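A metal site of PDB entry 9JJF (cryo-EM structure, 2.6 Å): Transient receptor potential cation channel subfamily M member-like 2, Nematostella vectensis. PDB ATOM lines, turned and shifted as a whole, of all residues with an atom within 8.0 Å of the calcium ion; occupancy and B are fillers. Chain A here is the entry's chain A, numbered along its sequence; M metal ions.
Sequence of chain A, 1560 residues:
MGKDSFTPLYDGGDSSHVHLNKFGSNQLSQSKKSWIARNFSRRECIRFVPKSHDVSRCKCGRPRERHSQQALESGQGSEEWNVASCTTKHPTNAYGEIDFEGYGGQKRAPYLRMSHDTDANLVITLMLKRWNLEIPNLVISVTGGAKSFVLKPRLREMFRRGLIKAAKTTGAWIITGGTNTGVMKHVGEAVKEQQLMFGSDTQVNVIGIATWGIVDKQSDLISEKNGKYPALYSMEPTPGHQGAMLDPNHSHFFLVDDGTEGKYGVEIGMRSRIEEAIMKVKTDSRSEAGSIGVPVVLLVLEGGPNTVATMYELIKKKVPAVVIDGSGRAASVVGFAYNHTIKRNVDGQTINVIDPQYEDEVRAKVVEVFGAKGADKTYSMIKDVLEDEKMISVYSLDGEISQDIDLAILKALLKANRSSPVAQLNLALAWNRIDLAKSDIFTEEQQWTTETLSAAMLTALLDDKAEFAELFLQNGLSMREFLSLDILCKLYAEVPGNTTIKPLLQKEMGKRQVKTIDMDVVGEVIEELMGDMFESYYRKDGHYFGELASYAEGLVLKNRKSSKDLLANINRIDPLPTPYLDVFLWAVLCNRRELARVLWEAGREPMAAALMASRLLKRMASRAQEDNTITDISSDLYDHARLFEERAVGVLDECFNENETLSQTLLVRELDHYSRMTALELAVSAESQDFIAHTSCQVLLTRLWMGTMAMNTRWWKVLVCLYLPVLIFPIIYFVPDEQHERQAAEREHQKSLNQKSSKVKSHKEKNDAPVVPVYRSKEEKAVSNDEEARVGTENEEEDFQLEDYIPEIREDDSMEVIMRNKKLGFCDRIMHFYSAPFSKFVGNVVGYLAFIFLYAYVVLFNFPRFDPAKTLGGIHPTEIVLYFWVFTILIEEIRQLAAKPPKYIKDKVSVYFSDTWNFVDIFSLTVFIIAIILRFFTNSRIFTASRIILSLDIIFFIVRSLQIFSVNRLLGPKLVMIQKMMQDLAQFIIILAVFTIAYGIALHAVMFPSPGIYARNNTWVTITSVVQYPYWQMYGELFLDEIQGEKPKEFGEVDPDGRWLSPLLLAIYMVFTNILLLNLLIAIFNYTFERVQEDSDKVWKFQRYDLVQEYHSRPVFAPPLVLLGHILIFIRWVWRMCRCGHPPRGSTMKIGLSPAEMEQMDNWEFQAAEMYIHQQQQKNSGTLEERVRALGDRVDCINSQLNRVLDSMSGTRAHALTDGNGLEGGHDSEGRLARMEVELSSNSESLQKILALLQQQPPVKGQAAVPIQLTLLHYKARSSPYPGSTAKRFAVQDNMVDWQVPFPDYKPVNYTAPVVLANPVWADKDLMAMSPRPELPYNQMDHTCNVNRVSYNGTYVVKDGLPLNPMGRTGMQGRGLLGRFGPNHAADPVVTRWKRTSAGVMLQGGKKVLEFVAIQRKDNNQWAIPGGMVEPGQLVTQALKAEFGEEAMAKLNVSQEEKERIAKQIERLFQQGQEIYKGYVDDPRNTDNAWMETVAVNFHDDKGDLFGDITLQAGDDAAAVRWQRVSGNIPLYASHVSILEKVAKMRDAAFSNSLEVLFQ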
ATOM      1  N   ILE A 889     -26.597 -24.443  37.778  1.00  0.00           N
ATOM      2  CA  ILE A 889     -27.252 -23.751  36.662  1.00  0.00           C
ATOM      3  C   ILE A 889     -26.593 -22.391  36.398  1.00  0.00           C
ATOM      4  O   ILE A 889     -26.403 -21.978  35.245  1.00  0.00           O
ATOM      5  CB  ILE A 889     -28.760 -23.612  36.937  1.00  0.00           C
ATOM      6  CG1 ILE A 889     -29.412 -24.989  37.046  1.00  0.00           C
ATOM      7  CG2 ILE A 889     -29.466 -22.839  35.845  1.00  0.00           C
ATOM      8  CD1 ILE A 889     -30.798 -24.958  37.633  1.00  0.00           C
ATOM      9  N   GLU A 892     -23.271 -22.953  34.797  1.00  0.00           N
ATOM     10  CA  GLU A 892     -23.567 -23.352  33.426  1.00  0.00           C
ATOM     11  C   GLU A 892     -23.836 -22.139  32.534  1.00  0.00           C
ATOM     12  O   GLU A 892     -23.312 -22.060  31.417  1.00  0.00           O
ATOM     13  CB  GLU A 892     -24.765 -24.308  33.411  1.00  0.00           C
ATOM     14  CG  GLU A 892     -25.296 -24.617  32.028  1.00  0.00           C
ATOM     15  CD  GLU A 892     -24.294 -25.318  31.137  1.00  0.00           C
ATOM     16  OE1 GLU A 892     -23.485 -26.116  31.644  1.00  0.00           O
ATOM     17  OE2 GLU A 892     -24.306 -25.021  29.924  1.00  0.00           O
ATOM     18  N   GLU A 893     -24.606 -21.172  33.030  1.00  0.00           N
ATOM     19  CA  GLU A 893     -24.875 -19.991  32.212  1.00  0.00           C
ATOM     20  C   GLU A 893     -23.663 -19.077  32.107  1.00  0.00           C
ATOM     21  O   GLU A 893     -23.468 -18.418  31.076  1.00  0.00           O
ATOM     22  CB  GLU A 893     -26.084 -19.244  32.755  1.00  0.00           C
ATOM     23  CG  GLU A 893     -27.363 -20.048  32.617  1.00  0.00           C
ATOM     24  CD  GLU A 893     -27.742 -20.298  31.176  1.00  0.00           C
ATOM     25  OE1 GLU A 893     -27.570 -19.397  30.332  1.00  0.00           O
ATOM     26  OE2 GLU A 893     -28.176 -21.434  30.866  1.00  0.00           O
ATOM     27  N   ARG A 895     -20.600 -20.276  31.998  1.00  0.00           N
ATOM     28  CA  ARG A 895     -19.817 -20.995  30.998  1.00  0.00           C
ATOM     29  C   ARG A 895     -20.365 -20.752  29.600  1.00  0.00           C
ATOM     30  O   ARG A 895     -19.590 -20.663  28.633  1.00  0.00           O
ATOM     31  CB  ARG A 895     -19.808 -22.481  31.334  1.00  0.00           C
ATOM     32  CG  ARG A 895     -18.728 -23.349  30.659  1.00  0.00           C
ATOM     33  CD  ARG A 895     -19.165 -23.925  29.332  1.00  0.00           C
ATOM     34  NE  ARG A 895     -20.420 -24.658  29.452  1.00  0.00           N
ATOM     35  CZ  ARG A 895     -21.247 -24.859  28.436  1.00  0.00           C
ATOM     36  NH1 ARG A 895     -20.972 -24.367  27.234  1.00  0.00           N
ATOM     37  NH2 ARG A 895     -22.372 -25.534  28.615  1.00  0.00           N
ATOM     38  N   GLN A 896     -21.689 -20.661  29.451  1.00  0.00           N
ATOM     39  CA  GLN A 896     -22.278 -20.378  28.143  1.00  0.00           C
ATOM     40  C   GLN A 896     -21.955 -18.959  27.691  1.00  0.00           C
ATOM     41  O   GLN A 896     -21.773 -18.716  26.497  1.00  0.00           O
ATOM     42  CB  GLN A 896     -23.785 -20.568  28.174  1.00  0.00           C
ATOM     43  CG  GLN A 896     -24.255 -21.997  28.340  1.00  0.00           C
ATOM     44  CD  GLN A 896     -25.759 -22.101  28.370  1.00  0.00           C
ATOM     45  OE1 GLN A 896     -26.455 -21.102  28.240  1.00  0.00           O
ATOM     46  NE2 GLN A 896     -26.253 -23.311  28.567  1.00  0.00           N
ATOM     47  N   LEU A 897     -21.885 -18.015  28.625  1.00  0.00           N
ATOM     48  CA  LEU A 897     -21.483 -16.653  28.293  1.00  0.00           C
ATOM     49  C   LEU A 897     -20.012 -16.600  27.898  1.00  0.00           C
ATOM     50  O   LEU A 897     -19.644 -15.954  26.910  1.00  0.00           O
ATOM     51  CB  LEU A 897     -21.749 -15.725  29.469  1.00  0.00           C
ATOM     52  CG  LEU A 897     -21.325 -14.266  29.299  1.00  0.00           C
ATOM     53  CD1 LEU A 897     -22.040 -13.632  28.144  1.00  0.00           C
ATOM     54  CD2 LEU A 897     -21.586 -13.494  30.574  1.00  0.00           C
ATOM     55  N   LYS A 900     -18.811 -18.051  24.278  1.00  0.00           N
ATOM     56  CA  LYS A 900     -19.295 -17.496  23.029  1.00  0.00           C
ATOM     57  C   LYS A 900     -18.135 -17.194  22.083  1.00  0.00           C
ATOM     58  O   LYS A 900     -17.027 -16.888  22.534  1.00  0.00           O
ATOM     59  CB  LYS A 900     -20.097 -16.225  23.300  1.00  0.00           C
ATOM     60  CG  LYS A 900     -21.369 -16.491  24.075  1.00  0.00           C
ATOM     61  CD  LYS A 900     -22.290 -17.360  23.254  1.00  0.00           C
ATOM     62  CE  LYS A 900     -23.602 -17.644  23.953  1.00  0.00           C
ATOM     63  NZ  LYS A 900     -24.472 -18.515  23.137  1.00  0.00           N
ATOM     64  N   TYR A 912     -24.975 -13.844  23.621  1.00  0.00           N
ATOM     65  CA  TYR A 912     -25.636 -14.629  24.658  1.00  0.00           C
ATOM     66  C   TYR A 912     -27.119 -14.307  24.759  1.00  0.00           C
ATOM     67  O   TYR A 912     -27.946 -15.217  24.867  1.00  0.00           O
ATOM     68  CB  TYR A 912     -24.941 -14.357  25.997  1.00  0.00           C
ATOM     69  CG  TYR A 912     -25.506 -15.115  27.157  1.00  0.00           C
ATOM     70  CD1 TYR A 912     -25.228 -16.461  27.353  1.00  0.00           C
ATOM     71  CD2 TYR A 912     -26.336 -14.479  28.081  1.00  0.00           C
ATOM     72  CE1 TYR A 912     -25.751 -17.152  28.420  1.00  0.00           C
ATOM     73  CE2 TYR A 912     -26.855 -15.155  29.149  1.00  0.00           C
ATOM     74  CZ  TYR A 912     -26.563 -16.488  29.308  1.00  0.00           C
ATOM     75  OH  TYR A 912     -27.091 -17.156  30.383  1.00  0.00           O
ATOM     76  N   ASP A 915     -30.842 -15.516  21.949  1.00  0.00           N
ATOM     77  CA  ASP A 915     -31.991 -16.369  22.208  1.00  0.00           C
ATOM     78  C   ASP A 915     -32.677 -15.970  23.506  1.00  0.00           C
ATOM     79  O   ASP A 915     -32.044 -15.475  24.445  1.00  0.00           O
ATOM     80  CB  ASP A 915     -31.594 -17.840  22.255  1.00  0.00           C
ATOM     81  CG  ASP A 915     -30.471 -18.134  23.225  1.00  0.00           C
ATOM     82  OD1 ASP A 915     -29.851 -17.173  23.743  1.00  0.00           O
ATOM     83  OD2 ASP A 915     -30.221 -19.326  23.494  1.00  0.00           O
ATOM     84  N   THR A 916     -33.986 -16.177  23.546  1.00  0.00           N
ATOM     85  CA  THR A 916     -34.780 -15.816  24.706  1.00  0.00           C
ATOM     86  C   THR A 916     -34.640 -16.819  25.838  1.00  0.00           C
ATOM     87  O   THR A 916     -35.046 -16.519  26.973  1.00  0.00           O
ATOM     88  CB  THR A 916     -36.239 -15.682  24.316  1.00  0.00           C
ATOM     89  OG1 THR A 916     -36.745 -16.950  23.882  1.00  0.00           O
ATOM     90  CG2 THR A 916     -36.379 -14.693  23.175  1.00  0.00           C
ATOM     91  N   TRP A 917     -34.086 -18.006  25.572  1.00  0.00           N
ATOM     92  CA  TRP A 917     -33.879 -18.982  26.629  1.00  0.00           C
ATOM     93  C   TRP A 917     -32.820 -18.522  27.606  1.00  0.00           C
ATOM     94  O   TRP A 917     -32.901 -18.821  28.801  1.00  0.00           O
ATOM     95  CB  TRP A 917     -33.504 -20.338  26.049  1.00  0.00           C
ATOM     96  CG  TRP A 917     -34.548 -20.957  25.185  1.00  0.00           C
ATOM     97  CD1 TRP A 917     -34.475 -21.141  23.840  1.00  0.00           C
ATOM     98  CD2 TRP A 917     -35.847 -21.405  25.588  1.00  0.00           C
ATOM     99  NE1 TRP A 917     -35.638 -21.710  23.388  1.00  0.00           N
ATOM    100  CE2 TRP A 917     -36.495 -21.881  24.445  1.00  0.00           C
ATOM    101  CE3 TRP A 917     -36.517 -21.467  26.817  1.00  0.00           C
ATOM    102  CZ2 TRP A 917     -37.773 -22.419  24.480  1.00  0.00           C
ATOM    103  CZ3 TRP A 917     -37.781 -21.986  26.845  1.00  0.00           C
ATOM    104  CH2 TRP A 917     -38.402 -22.460  25.690  1.00  0.00           C
ATOM    105  N   ASN A 918     -31.836 -17.758  27.140  1.00  0.00           N
ATOM    106  CA  ASN A 918     -30.887 -17.129  28.049  1.00  0.00           C
ATOM    107  C   ASN A 918     -31.543 -16.032  28.871  1.00  0.00           C
ATOM    108  O   ASN A 918     -31.145 -15.809  30.015  1.00  0.00           O
ATOM    109  CB  ASN A 918     -29.689 -16.582  27.287  1.00  0.00           C
ATOM    110  CG  ASN A 918     -28.791 -17.675  26.781  1.00  0.00           C
ATOM    111  OD1 ASN A 918     -28.565 -18.662  27.456  1.00  0.00           O
ATOM    112  ND2 ASN A 918     -28.264 -17.491  25.579  1.00  0.00           N
ATOM    113  N   PHE A 919     -32.549 -15.345  28.317  1.00  0.00           N
ATOM    114  CA  PHE A 919     -33.314 -14.391  29.129  1.00  0.00           C
ATOM    115  C   PHE A 919     -34.079 -15.094  30.236  1.00  0.00           C
ATOM    116  O   PHE A 919     -34.115 -14.621  31.367  1.00  0.00           O
ATOM    117  CB  PHE A 919     -34.297 -13.602  28.255  1.00  0.00           C
ATOM    118  CG  PHE A 919     -33.660 -12.533  27.436  1.00  0.00           C
ATOM    119  CD1 PHE A 919     -33.314 -11.311  28.010  1.00  0.00           C
ATOM    120  CD2 PHE A 919     -33.435 -12.717  26.085  1.00  0.00           C
ATOM    121  CE1 PHE A 919     -32.743 -10.318  27.255  1.00  0.00           C
ATOM    122  CE2 PHE A 919     -32.869 -11.715  25.329  1.00  0.00           C
ATOM    123  CZ  PHE A 919     -32.521 -10.516  25.905  1.00  0.00           C
ATOM    124  N   VAL A 920     -34.689 -16.246  29.925  1.00  0.00           N
ATOM    125  CA  VAL A 920     -35.400 -17.020  30.935  1.00  0.00           C
ATOM    126  C   VAL A 920     -34.435 -17.554  31.987  1.00  0.00           C
ATOM    127  O   VAL A 920     -34.724 -17.524  33.195  1.00  0.00           O
ATOM    128  CB  VAL A 920     -36.211 -18.147  30.268  1.00  0.00           C
ATOM    129  CG1 VAL A 920     -36.931 -18.993  31.308  1.00  0.00           C
ATOM    130  CG2 VAL A 920     -37.202 -17.568  29.280  1.00  0.00           C
ATOM    131  N   ASP A 921     -33.247 -17.991  31.545  1.00  0.00           N
ATOM    132  CA  ASP A 921     -32.192 -18.450  32.456  1.00  0.00           C
ATOM    133  C   ASP A 921     -31.740 -17.344  33.411  1.00  0.00           C
ATOM    134  O   ASP A 921     -31.717 -17.549  34.626  1.00  0.00           O
ATOM    135  CB  ASP A 921     -30.997 -18.961  31.652  1.00  0.00           C
ATOM    136  CG  ASP A 921     -31.203 -20.341  31.103  1.00  0.00           C
ATOM    137  OD1 ASP A 921     -31.814 -21.166  31.811  1.00  0.00           O
ATOM    138  OD2 ASP A 921     -30.786 -20.600  29.960  1.00  0.00           O
ATOM    139  N   ILE A 922     -31.375 -16.182  32.872  1.00  0.00           N
ATOM    140  CA  ILE A 922     -30.866 -15.089  33.708  1.00  0.00           C
ATOM    141  C   ILE A 922     -31.959 -14.530  34.605  1.00  0.00           C
ATOM    142  O   ILE A 922     -31.690 -14.204  35.771  1.00  0.00           O
ATOM    143  CB  ILE A 922     -30.219 -14.019  32.809  1.00  0.00           C
ATOM    144  CG1 ILE A 922     -28.979 -14.608  32.125  1.00  0.00           C
ATOM    145  CG2 ILE A 922     -29.806 -12.782  33.591  1.00  0.00           C
ATOM    146  CD1 ILE A 922     -27.939 -15.138  33.084  1.00  0.00           C
ATOM    147  N   ARG A 960     -38.390 -22.597  31.380  1.00  0.00           N
ATOM    148  CA  ARG A 960     -37.103 -22.925  30.768  1.00  0.00           C
ATOM    149  C   ARG A 960     -37.044 -24.374  30.292  1.00  0.00           C
ATOM    150  O   ARG A 960     -36.427 -24.662  29.264  1.00  0.00           O
ATOM    151  CB  ARG A 960     -35.967 -22.623  31.731  1.00  0.00           C
ATOM    152  CG  ARG A 960     -34.590 -22.839  31.145  1.00  0.00           C
ATOM    153  CD  ARG A 960     -34.410 -21.925  29.947  1.00  0.00           C
ATOM    154  NE  ARG A 960     -33.156 -22.185  29.240  1.00  0.00           N
ATOM    155  CZ  ARG A 960     -33.027 -23.072  28.261  1.00  0.00           C
ATOM    156  NH1 ARG A 960     -34.069 -23.791  27.881  1.00  0.00           N
ATOM    157  NH2 ARG A 960     -31.853 -23.249  27.675  1.00  0.00           N
ATOM    158  N   GLN A 963     -37.604 -26.227  26.022  1.00  0.00           N
ATOM    159  CA  GLN A 963     -36.651 -26.617  24.984  1.00  0.00           C
ATOM    160  C   GLN A 963     -36.376 -28.121  25.016  1.00  0.00           C
ATOM    161  O   GLN A 963     -35.980 -28.691  23.998  1.00  0.00           O
ATOM    162  CB  GLN A 963     -35.364 -25.814  25.146  1.00  0.00           C
ATOM    163  CG  GLN A 963     -34.465 -25.833  23.927  1.00  0.00           C
ATOM    164  CD  GLN A 963     -33.255 -24.972  24.084  1.00  0.00           C
ATOM    165  OE1 GLN A 963     -33.006 -24.415  25.154  1.00  0.00           O
ATOM    166  NE2 GLN A 963     -32.502 -24.823  23.005  1.00  0.00           N
ATOM    167  N   GLU A1110     -27.398 -26.044  21.768  1.00  0.00           N
ATOM    168  CA  GLU A1110     -27.405 -25.856  23.217  1.00  0.00           C
ATOM    169  C   GLU A1110     -26.891 -27.061  23.986  1.00  0.00           C
ATOM    170  O   GLU A1110     -26.704 -26.945  25.203  1.00  0.00           O
ATOM    171  CB  GLU A1110     -28.807 -25.500  23.688  1.00  0.00           C
ATOM    172  CG  GLU A1110     -29.213 -24.085  23.293  1.00  0.00           C
ATOM    173  CD  GLU A1110     -28.379 -23.022  23.990  1.00  0.00           C
ATOM    174  OE1 GLU A1110     -28.010 -23.220  25.165  1.00  0.00           O
ATOM    175  OE2 GLU A1110     -28.063 -21.998  23.345  1.00  0.00           O
ATOM    176  N   ARG A1114     -22.124 -28.357  26.069  1.00  0.00           N
ATOM    177  CA  ARG A1114     -22.211 -28.785  27.464  1.00  0.00           C
ATOM    178  C   ARG A1114     -20.988 -29.623  27.848  1.00  0.00           C
ATOM    179  O   ARG A1114     -20.323 -30.194  26.986  1.00  0.00           O
ATOM    180  CB  ARG A1114     -23.488 -29.597  27.672  1.00  0.00           C
ATOM    181  CG  ARG A1114     -24.790 -28.878  27.413  1.00  0.00           C
ATOM    182  CD  ARG A1114     -25.026 -27.790  28.407  1.00  0.00           C
ATOM    183  NE  ARG A1114     -26.321 -27.170  28.225  1.00  0.00           N
ATOM    184  CZ  ARG A1114     -27.419 -27.530  28.888  1.00  0.00           C
ATOM    185  NH1 ARG A1114     -27.354 -28.501  29.775  1.00  0.00           N
ATOM    186  NH2 ARG A1114     -28.563 -26.908  28.659  1.00  0.00           N
HETATM  187 CA    CA M   1     -28.971 -21.066  28.269  1.00  0.00          CA
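ND2 of Asn 918 sits at hydrogen-bond distance from O of Tyr 912 (2.4 Å). NE2 of Gln 896 is in hydrogen-bond range of OE2 of Glu 892, 2.9 Å away. The backbone carbonyl oxygen (O) of Glu 1110 sits at hydrogen-bond distance from the guanidinium group (NE) of Arg 1114 (3.1 Å). The guanidinium group of Arg 960 lies within hydrogen-bond range of the side-chain amide oxygen of Gln 963, at 3.0 Å. NE of Arg 960 is in salt-bridge range of OD1 of Asp 921. The side-chain amide nitrogen (ND2) of Asn 918 lies within hydrogen-bond range of the side-chain carboxylate (OD1) of Asp 915 (2.4 Å). The guanidinium group of Arg 960 lies within hydrogen-bond range of the backbone carbonyl oxygen of Trp 917.
Arg 960 touches the calcium ion (NH2 to CA, 3.7 Å). OE1 of Glu 1110 touches the calcium ion (3.9 Å). Within 4 Å of the calcium ion: Glu 893, Gln 896, Asn 918, Asp 921, Arg 960 and Glu 1110.
The calcium ion is bound by the side-chain amide oxygen of Gln 896, the side-chain carboxylate of Asp 921, the side-chain amide oxygen of Asn 918 and the side-chain carboxylate of Glu 893. Slightly farther from the calcium ion lies OE1 of Glu 893 (3.0 Å).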
